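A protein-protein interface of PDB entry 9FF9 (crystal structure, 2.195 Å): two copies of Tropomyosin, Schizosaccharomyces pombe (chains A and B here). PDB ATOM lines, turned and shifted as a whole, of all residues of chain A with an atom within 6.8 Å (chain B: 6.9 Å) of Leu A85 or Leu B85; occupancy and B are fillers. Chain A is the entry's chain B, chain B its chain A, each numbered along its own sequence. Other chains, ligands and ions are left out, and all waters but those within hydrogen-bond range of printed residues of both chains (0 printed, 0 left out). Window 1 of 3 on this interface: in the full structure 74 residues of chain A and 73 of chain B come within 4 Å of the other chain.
The backbone carbonyl oxygen of Ala A82 sits at hydrogen-bond distance from the side-chain hydroxyl of Ser A86 (3.4 Å).
Among the printed residues, merely in contact across the chains: Ala A82 with Ala B82, Ala A82 with Leu B85, Leu A85 with Ala B82, Leu A85 with Leu B85, Leu A85 with Ser B86, Ser A86 with Leu B85 and Val A89 with Val B89.
Of the printed residues of chain A, Leu B85 touches Ala A82, Leu A85 and Ser A86. Of the printed residues of chain A, Val B89 touches Val A89 (3.6 Å). Printed residues of chain A within 4 Å of Ala B82: Ala A82 and Leu A85. Of the printed residues of chain B, Ser A86 touches Leu B85. Glu A81 touches none of the printed residues of chain B. The nearest printed residue of chain A that does not touch Leu B85 is Val A89 (4.1 Å). The nearest printed residue of chain A that does not touch Ala B82 is Glu A81 (5.1 Å).
Of the 11 printed residues of chain A, 4 touch a printed residue of chain B. Hydrophobic or aromatic side chains of chain A within 4 Å of the printed part of chain B: Ala A82, Leu A85 and Val A89. Of the 12 printed residues of chain B, 4 touch a printed residue of chain A. Printed residues of chain B that touch a printed residue of chain A: Ala B82, Leu B85, Ser B86 and Val B89.
Ala A82 touches its own counterpart, Ala B82. Leu A85 touches its own counterpart, Leu B85. Leu A85 touches Ser B86, and with the chains exchanged Ser A86 touches Leu B85. Val A89 touches its own counterpart, Val B89. Positions printed for both chains: 80, 81, 82, 83, 84, 85, 86, 87, 88, 89 and 90. Of the 7 pairs that touch across the chains among the printed residues, 7 have their exchanged pair printed and touching as well.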
ATOM      1  N   THR A  80       7.846 -36.835 -18.600  1.00  0.00           N
ATOM      2  CA  THR A  80       8.870 -35.796 -18.474  1.00  0.00           C
ATOM      3  C   THR A  80       8.519 -34.575 -19.326  1.00  0.00           C
ATOM      4  O   THR A  80       8.621 -33.421 -18.870  1.00  0.00           O
ATOM      5  CB  THR A  80      10.240 -36.355 -18.866  1.00  0.00           C
ATOM      6  OG1 THR A  80      10.681 -37.290 -17.873  1.00  0.00           O
ATOM      7  CG2 THR A  80      11.260 -35.231 -18.991  1.00  0.00           C
ATOM      8  N   GLU A  81       8.102 -34.816 -20.575  1.00  0.00           N
ATOM      9  CA  GLU A  81       7.694 -33.711 -21.440  1.00  0.00           C
ATOM     10  C   GLU A  81       6.524 -32.938 -20.837  1.00  0.00           C
ATOM     11  O   GLU A  81       6.446 -31.711 -20.964  1.00  0.00           O
ATOM     12  CB  GLU A  81       7.332 -34.240 -22.827  1.00  0.00           C
ATOM     13  CG  GLU A  81       6.998 -33.148 -23.825  1.00  0.00           C
ATOM     14  CD  GLU A  81       8.171 -32.219 -24.079  1.00  0.00           C
ATOM     15  OE1 GLU A  81       9.289 -32.726 -24.311  1.00  0.00           O
ATOM     16  OE2 GLU A  81       7.978 -30.985 -24.032  1.00  0.00           O
ATOM     17  N   ALA A  82       5.610 -33.644 -20.167  1.00  0.00           N
ATOM     18  CA  ALA A  82       4.464 -32.988 -19.545  1.00  0.00           C
ATOM     19  C   ALA A  82       4.895 -32.114 -18.377  1.00  0.00           C
ATOM     20  O   ALA A  82       4.350 -31.023 -18.176  1.00  0.00           O
ATOM     21  CB  ALA A  82       3.451 -34.033 -19.081  1.00  0.00           C
ATOM     22  N   GLU A  83       5.855 -32.590 -17.581  1.00  0.00           N
ATOM     23  CA  GLU A  83       6.415 -31.761 -16.518  1.00  0.00           C
ATOM     24  C   GLU A  83       6.986 -30.464 -17.081  1.00  0.00           C
ATOM     25  O   GLU A  83       6.701 -29.364 -16.576  1.00  0.00           O
ATOM     26  CB  GLU A  83       7.493 -32.539 -15.761  1.00  0.00           C
ATOM     27  CG  GLU A  83       8.382 -31.675 -14.880  1.00  0.00           C
ATOM     28  CD  GLU A  83       9.553 -32.443 -14.303  1.00  0.00           C
ATOM     29  OE1 GLU A  83       9.564 -33.685 -14.414  1.00  0.00           O
ATOM     30  OE2 GLU A  83      10.467 -31.801 -13.741  1.00  0.00           O
ATOM     31  N   GLN A  84       7.798 -30.575 -18.136  1.00  0.00           N
ATOM     32  CA  GLN A  84       8.383 -29.375 -18.733  1.00  0.00           C
ATOM     33  C   GLN A  84       7.305 -28.446 -19.288  1.00  0.00           C
ATOM     34  O   GLN A  84       7.396 -27.217 -19.152  1.00  0.00           O
ATOM     35  CB  GLN A  84       9.386 -29.758 -19.821  1.00  0.00           C
ATOM     36  CG  GLN A  84      10.611 -30.487 -19.291  1.00  0.00           C
ATOM     37  CD  GLN A  84      11.299 -29.728 -18.168  1.00  0.00           C
ATOM     38  OE1 GLN A  84      11.560 -30.280 -17.099  1.00  0.00           O
ATOM     39  NE2 GLN A  84      11.595 -28.454 -18.408  1.00  0.00           N
ATOM     40  N   LEU A  85       6.268 -29.020 -19.905  1.00  0.00           N
ATOM     41  CA  LEU A  85       5.183 -28.212 -20.450  1.00  0.00           C
ATOM     42  C   LEU A  85       4.429 -27.479 -19.347  1.00  0.00           C
ATOM     43  O   LEU A  85       4.035 -26.321 -19.521  1.00  0.00           O
ATOM     44  CB  LEU A  85       4.233 -29.096 -21.256  1.00  0.00           C
ATOM     45  CG  LEU A  85       4.226 -28.912 -22.774  1.00  0.00           C
ATOM     46  CD1 LEU A  85       5.640 -28.774 -23.318  1.00  0.00           C
ATOM     47  CD2 LEU A  85       3.514 -30.080 -23.435  1.00  0.00           C
ATOM     48  N   SER A  86       4.216 -28.138 -18.206  1.00  0.00           N
ATOM     49  CA  SER A  86       3.565 -27.472 -17.082  1.00  0.00           C
ATOM     50  C   SER A  86       4.405 -26.309 -16.574  1.00  0.00           C
ATOM     51  O   SER A  86       3.875 -25.224 -16.298  1.00  0.00           O
ATOM     52  CB  SER A  86       3.300 -28.467 -15.952  1.00  0.00           C
ATOM     53  OG  SER A  86       2.180 -29.285 -16.238  1.00  0.00           O
ATOM     54  N   ARG A  87       5.718 -26.521 -16.432  1.00  0.00           N
ATOM     55  CA  ARG A  87       6.598 -25.426 -16.025  1.00  0.00           C
ATOM     56  C   ARG A  87       6.463 -24.235 -16.969  1.00  0.00           C
ATOM     57  O   ARG A  87       6.295 -23.085 -16.531  1.00  0.00           O
ATOM     58  CB  ARG A  87       8.050 -25.902 -15.972  1.00  0.00           C
ATOM     59  CG  ARG A  87       8.329 -26.979 -14.935  1.00  0.00           C
ATOM     60  CD  ARG A  87       9.825 -27.220 -14.783  1.00  0.00           C
ATOM     61  NE  ARG A  87      10.522 -26.027 -14.316  1.00  0.00           N
ATOM     62  CZ  ARG A  87      11.836 -25.928 -14.175  1.00  0.00           C
ATOM     63  NH1 ARG A  87      12.641 -26.937 -14.465  1.00  0.00           N
ATOM     64  NH2 ARG A  87      12.358 -24.787 -13.735  1.00  0.00           N
ATOM     65  N   LYS A  88       6.529 -24.499 -18.278  1.00  0.00           N
ATOM     66  CA  LYS A  88       6.452 -23.415 -19.254  1.00  0.00           C
ATOM     67  C   LYS A  88       5.098 -22.714 -19.205  1.00  0.00           C
ATOM     68  O   LYS A  88       5.026 -21.483 -19.304  1.00  0.00           O
ATOM     69  CB  LYS A  88       6.736 -23.947 -20.658  1.00  0.00           C
ATOM     70  CG  LYS A  88       8.149 -24.487 -20.828  1.00  0.00           C
ATOM     71  CD  LYS A  88       9.191 -23.432 -20.481  1.00  0.00           C
ATOM     72  CE  LYS A  88      10.574 -24.046 -20.329  1.00  0.00           C
ATOM     73  NZ  LYS A  88      10.629 -25.003 -19.186  1.00  0.00           N
ATOM     74  N   VAL A  89       4.012 -23.478 -19.047  1.00  0.00           N
ATOM     75  CA  VAL A  89       2.681 -22.878 -18.982  1.00  0.00           C
ATOM     76  C   VAL A  89       2.565 -21.958 -17.776  1.00  0.00           C
ATOM     77  O   VAL A  89       2.030 -20.845 -17.874  1.00  0.00           O
ATOM     78  CB  VAL A  89       1.596 -23.972 -18.963  1.00  0.00           C
ATOM     79  CG1 VAL A  89       0.261 -23.394 -18.517  1.00  0.00           C
ATOM     80  CG2 VAL A  89       1.458 -24.607 -20.332  1.00  0.00           C
ATOM     81  N   GLU A  90       3.066 -22.400 -16.618  1.00  0.00           N
ATOM     82  CA  GLU A  90       2.987 -21.561 -15.424  1.00  0.00           C
ATOM     83  C   GLU A  90       3.792 -20.277 -15.600  1.00  0.00           C
ATOM     84  O   GLU A  90       3.312 -19.182 -15.264  1.00  0.00           O
ATOM     85  CB  GLU A  90       3.468 -22.335 -14.196  1.00  0.00           C
ATOM     86  CG  GLU A  90       2.721 -23.640 -13.915  1.00  0.00           C
ATOM     87  CD  GLU A  90       1.211 -23.487 -13.923  1.00  0.00           C
ATOM     88  OE1 GLU A  90       0.603 -23.563 -15.012  1.00  0.00           O
ATOM     89  OE2 GLU A  90       0.628 -23.296 -12.835  1.00  0.00           O
ATOM     90  N   LYS B  79      -0.449 -38.908 -21.781  1.00  0.00           N
ATOM     91  CA  LYS B  79      -0.152 -38.386 -23.111  1.00  0.00           C
ATOM     92  C   LYS B  79      -1.262 -37.464 -23.597  1.00  0.00           C
ATOM     93  O   LYS B  79      -0.989 -36.417 -24.198  1.00  0.00           O
ATOM     94  CB  LYS B  79       0.065 -39.530 -24.101  1.00  0.00           C
ATOM     95  CG  LYS B  79       0.384 -39.047 -25.508  1.00  0.00           C
ATOM     96  CD  LYS B  79       0.371 -40.174 -26.524  1.00  0.00           C
ATOM     97  CE  LYS B  79       0.622 -39.643 -27.930  1.00  0.00           C
ATOM     98  NZ  LYS B  79       0.521 -40.709 -28.967  1.00  0.00           N
ATOM     99  N   THR B  80      -2.518 -37.835 -23.342  1.00  0.00           N
ATOM    100  CA  THR B  80      -3.638 -36.985 -23.728  1.00  0.00           C
ATOM    101  C   THR B  80      -3.602 -35.649 -22.997  1.00  0.00           C
ATOM    102  O   THR B  80      -4.025 -34.628 -23.549  1.00  0.00           O
ATOM    103  CB  THR B  80      -4.961 -37.703 -23.453  1.00  0.00           C
ATOM    104  OG1 THR B  80      -4.909 -39.034 -23.983  1.00  0.00           O
ATOM    105  CG2 THR B  80      -6.118 -36.952 -24.095  1.00  0.00           C
ATOM    106  N   GLU B  81      -3.094 -35.632 -21.763  1.00  0.00           N
ATOM    107  CA  GLU B  81      -3.057 -34.390 -20.998  1.00  0.00           C
ATOM    108  C   GLU B  81      -1.947 -33.469 -21.489  1.00  0.00           C
ATOM    109  O   GLU B  81      -2.162 -32.261 -21.645  1.00  0.00           O
ATOM    110  CB  GLU B  81      -2.888 -34.693 -19.507  1.00  0.00           C
ATOM    111  CG  GLU B  81      -2.890 -33.455 -18.626  1.00  0.00           C
ATOM    112  CD  GLU B  81      -4.181 -32.661 -18.728  1.00  0.00           C
ATOM    113  OE1 GLU B  81      -5.254 -33.281 -18.890  1.00  0.00           O
ATOM    114  OE2 GLU B  81      -4.124 -31.416 -18.652  1.00  0.00           O
ATOM    115  N   ALA B  82      -0.758 -34.019 -21.744  1.00  0.00           N
ATOM    116  CA  ALA B  82       0.354 -33.184 -22.189  1.00  0.00           C
ATOM    117  C   ALA B  82       0.112 -32.627 -23.584  1.00  0.00           C
ATOM    118  O   ALA B  82       0.514 -31.496 -23.884  1.00  0.00           O
ATOM    119  CB  ALA B  82       1.659 -33.973 -22.159  1.00  0.00           C
ATOM    120  N   GLU B  83      -0.524 -33.411 -24.459  1.00  0.00           N
ATOM    121  CA  GLU B  83      -0.834 -32.915 -25.794  1.00  0.00           C
ATOM    122  C   GLU B  83      -1.815 -31.752 -25.737  1.00  0.00           C
ATOM    123  O   GLU B  83      -1.793 -30.877 -26.610  1.00  0.00           O
ATOM    124  CB  GLU B  83      -1.383 -34.047 -26.664  1.00  0.00           C
ATOM    125  CG  GLU B  83      -1.444 -33.715 -28.149  1.00  0.00           C
ATOM    126  CD  GLU B  83      -1.731 -34.934 -29.006  1.00  0.00           C
ATOM    127  OE1 GLU B  83      -1.887 -36.036 -28.440  1.00  0.00           O
ATOM    128  OE2 GLU B  83      -1.796 -34.790 -30.245  1.00  0.00           O
ATOM    129  N   GLN B  84      -2.680 -31.721 -24.720  1.00  0.00           N
ATOM    130  CA  GLN B  84      -3.504 -30.539 -24.493  1.00  0.00           C
ATOM    131  C   GLN B  84      -2.713 -29.430 -23.813  1.00  0.00           C
ATOM    132  O   GLN B  84      -3.015 -28.249 -24.012  1.00  0.00           O
ATOM    133  CB  GLN B  84      -4.738 -30.899 -23.662  1.00  0.00           C
ATOM    134  CG  GLN B  84      -5.609 -31.996 -24.266  1.00  0.00           C
ATOM    135  CD  GLN B  84      -6.139 -31.649 -25.646  1.00  0.00           C
ATOM    136  OE1 GLN B  84      -6.383 -30.483 -25.959  1.00  0.00           O
ATOM    137  NE2 GLN B  84      -6.322 -32.666 -26.481  1.00  0.00           N
ATOM    138  N   LEU B  85      -1.704 -29.786 -23.012  1.00  0.00           N
ATOM    139  CA  LEU B  85      -0.818 -28.774 -22.444  1.00  0.00           C
ATOM    140  C   LEU B  85       0.036 -28.124 -23.525  1.00  0.00           C
ATOM    141  O   LEU B  85       0.327 -26.924 -23.457  1.00  0.00           O
ATOM    142  CB  LEU B  85       0.069 -29.394 -21.365  1.00  0.00           C
ATOM    143  CG  LEU B  85      -0.347 -29.193 -19.907  1.00  0.00           C
ATOM    144  CD1 LEU B  85      -1.760 -29.701 -19.667  1.00  0.00           C
ATOM    145  CD2 LEU B  85       0.639 -29.888 -18.983  1.00  0.00           C
ATOM    146  N   SER B  86       0.454 -28.906 -24.525  1.00  0.00           N
ATOM    147  CA  SER B  86       1.187 -28.340 -25.653  1.00  0.00           C
ATOM    148  C   SER B  86       0.336 -27.337 -26.419  1.00  0.00           C
ATOM    149  O   SER B  86       0.862 -26.352 -26.950  1.00  0.00           O
ATOM    150  CB  SER B  86       1.664 -29.457 -26.582  1.00  0.00           C
ATOM    151  OG  SER B  86       2.328 -28.931 -27.717  1.00  0.00           O
ATOM    152  N   ARG B  87      -0.976 -27.570 -26.486  1.00  0.00           N
ATOM    153  CA  ARG B  87      -1.870 -26.582 -27.077  1.00  0.00           C
ATOM    154  C   ARG B  87      -2.000 -25.349 -26.193  1.00  0.00           C
ATOM    155  O   ARG B  87      -2.188 -24.239 -26.703  1.00  0.00           O
ATOM    156  CB  ARG B  87      -3.246 -27.195 -27.326  1.00  0.00           C
ATOM    157  CG  ARG B  87      -3.269 -28.320 -28.344  1.00  0.00           C
ATOM    158  CD  ARG B  87      -4.705 -28.674 -28.675  1.00  0.00           C
ATOM    159  NE  ARG B  87      -5.470 -27.472 -28.984  1.00  0.00           N
ATOM    160  CZ  ARG B  87      -6.792 -27.388 -28.939  1.00  0.00           C
ATOM    161  NH1 ARG B  87      -7.539 -28.426 -28.600  1.00  0.00           N
ATOM    162  NH2 ARG B  87      -7.379 -26.232 -29.236  1.00  0.00           N
ATOM    163  N   LYS B  88      -1.910 -25.524 -24.872  1.00  0.00           N
ATOM    164  CA  LYS B  88      -1.992 -24.381 -23.969  1.00  0.00           C
ATOM    165  C   LYS B  88      -0.761 -23.491 -24.082  1.00  0.00           C
ATOM    166  O   LYS B  88      -0.858 -22.276 -23.872  1.00  0.00           O
ATOM    167  CB  LYS B  88      -2.181 -24.861 -22.530  1.00  0.00           C
ATOM    168  CG  LYS B  88      -3.510 -25.561 -22.289  1.00  0.00           C
ATOM    169  CD  LYS B  88      -3.615 -26.103 -20.873  1.00  0.00           C
ATOM    170  CE  LYS B  88      -4.954 -26.790 -20.643  1.00  0.00           C
ATOM    171  NZ  LYS B  88      -5.168 -27.929 -21.578  1.00  0.00           N
ATOM    172  N   VAL B  89       0.396 -24.068 -24.414  1.00  0.00           N
ATOM    173  CA  VAL B  89       1.584 -23.254 -24.653  1.00  0.00           C
ATOM    174  C   VAL B  89       1.396 -22.391 -25.893  1.00  0.00           C
ATOM    175  O   VAL B  89       1.819 -21.229 -25.927  1.00  0.00           O
ATOM    176  CB  VAL B  89       2.833 -24.148 -24.768  1.00  0.00           C
ATOM    177  CG1 VAL B  89       4.083 -23.296 -24.944  1.00  0.00           C
ATOM    178  CG2 VAL B  89       2.966 -25.043 -23.549  1.00  0.00           C
ATOM    179  N   GLU B  90       0.756 -22.941 -26.929  1.00  0.00           N
ATOM    180  CA  GLU B  90       0.526 -22.172 -28.149  1.00  0.00           C
ATOM    181  C   GLU B  90      -0.439 -21.018 -27.902  1.00  0.00           C
ATOM    182  O   GLU B  90      -0.252 -19.922 -28.439  1.00  0.00           O
ATOM    183  CB  GLU B  90       0.000 -23.084 -29.257  1.00  0.00           C
ATOM    184  CG  GLU B  90       0.952 -24.204 -29.662  1.00  0.00           C
ATOM    185  CD  GLU B  90       2.183 -23.702 -30.396  1.00  0.00           C
ATOM    186  OE1 GLU B  90       2.132 -22.591 -30.968  1.00  0.00           O
ATOM    187  OE2 GLU B  90       3.205 -24.420 -30.403  1.00  0.00           O
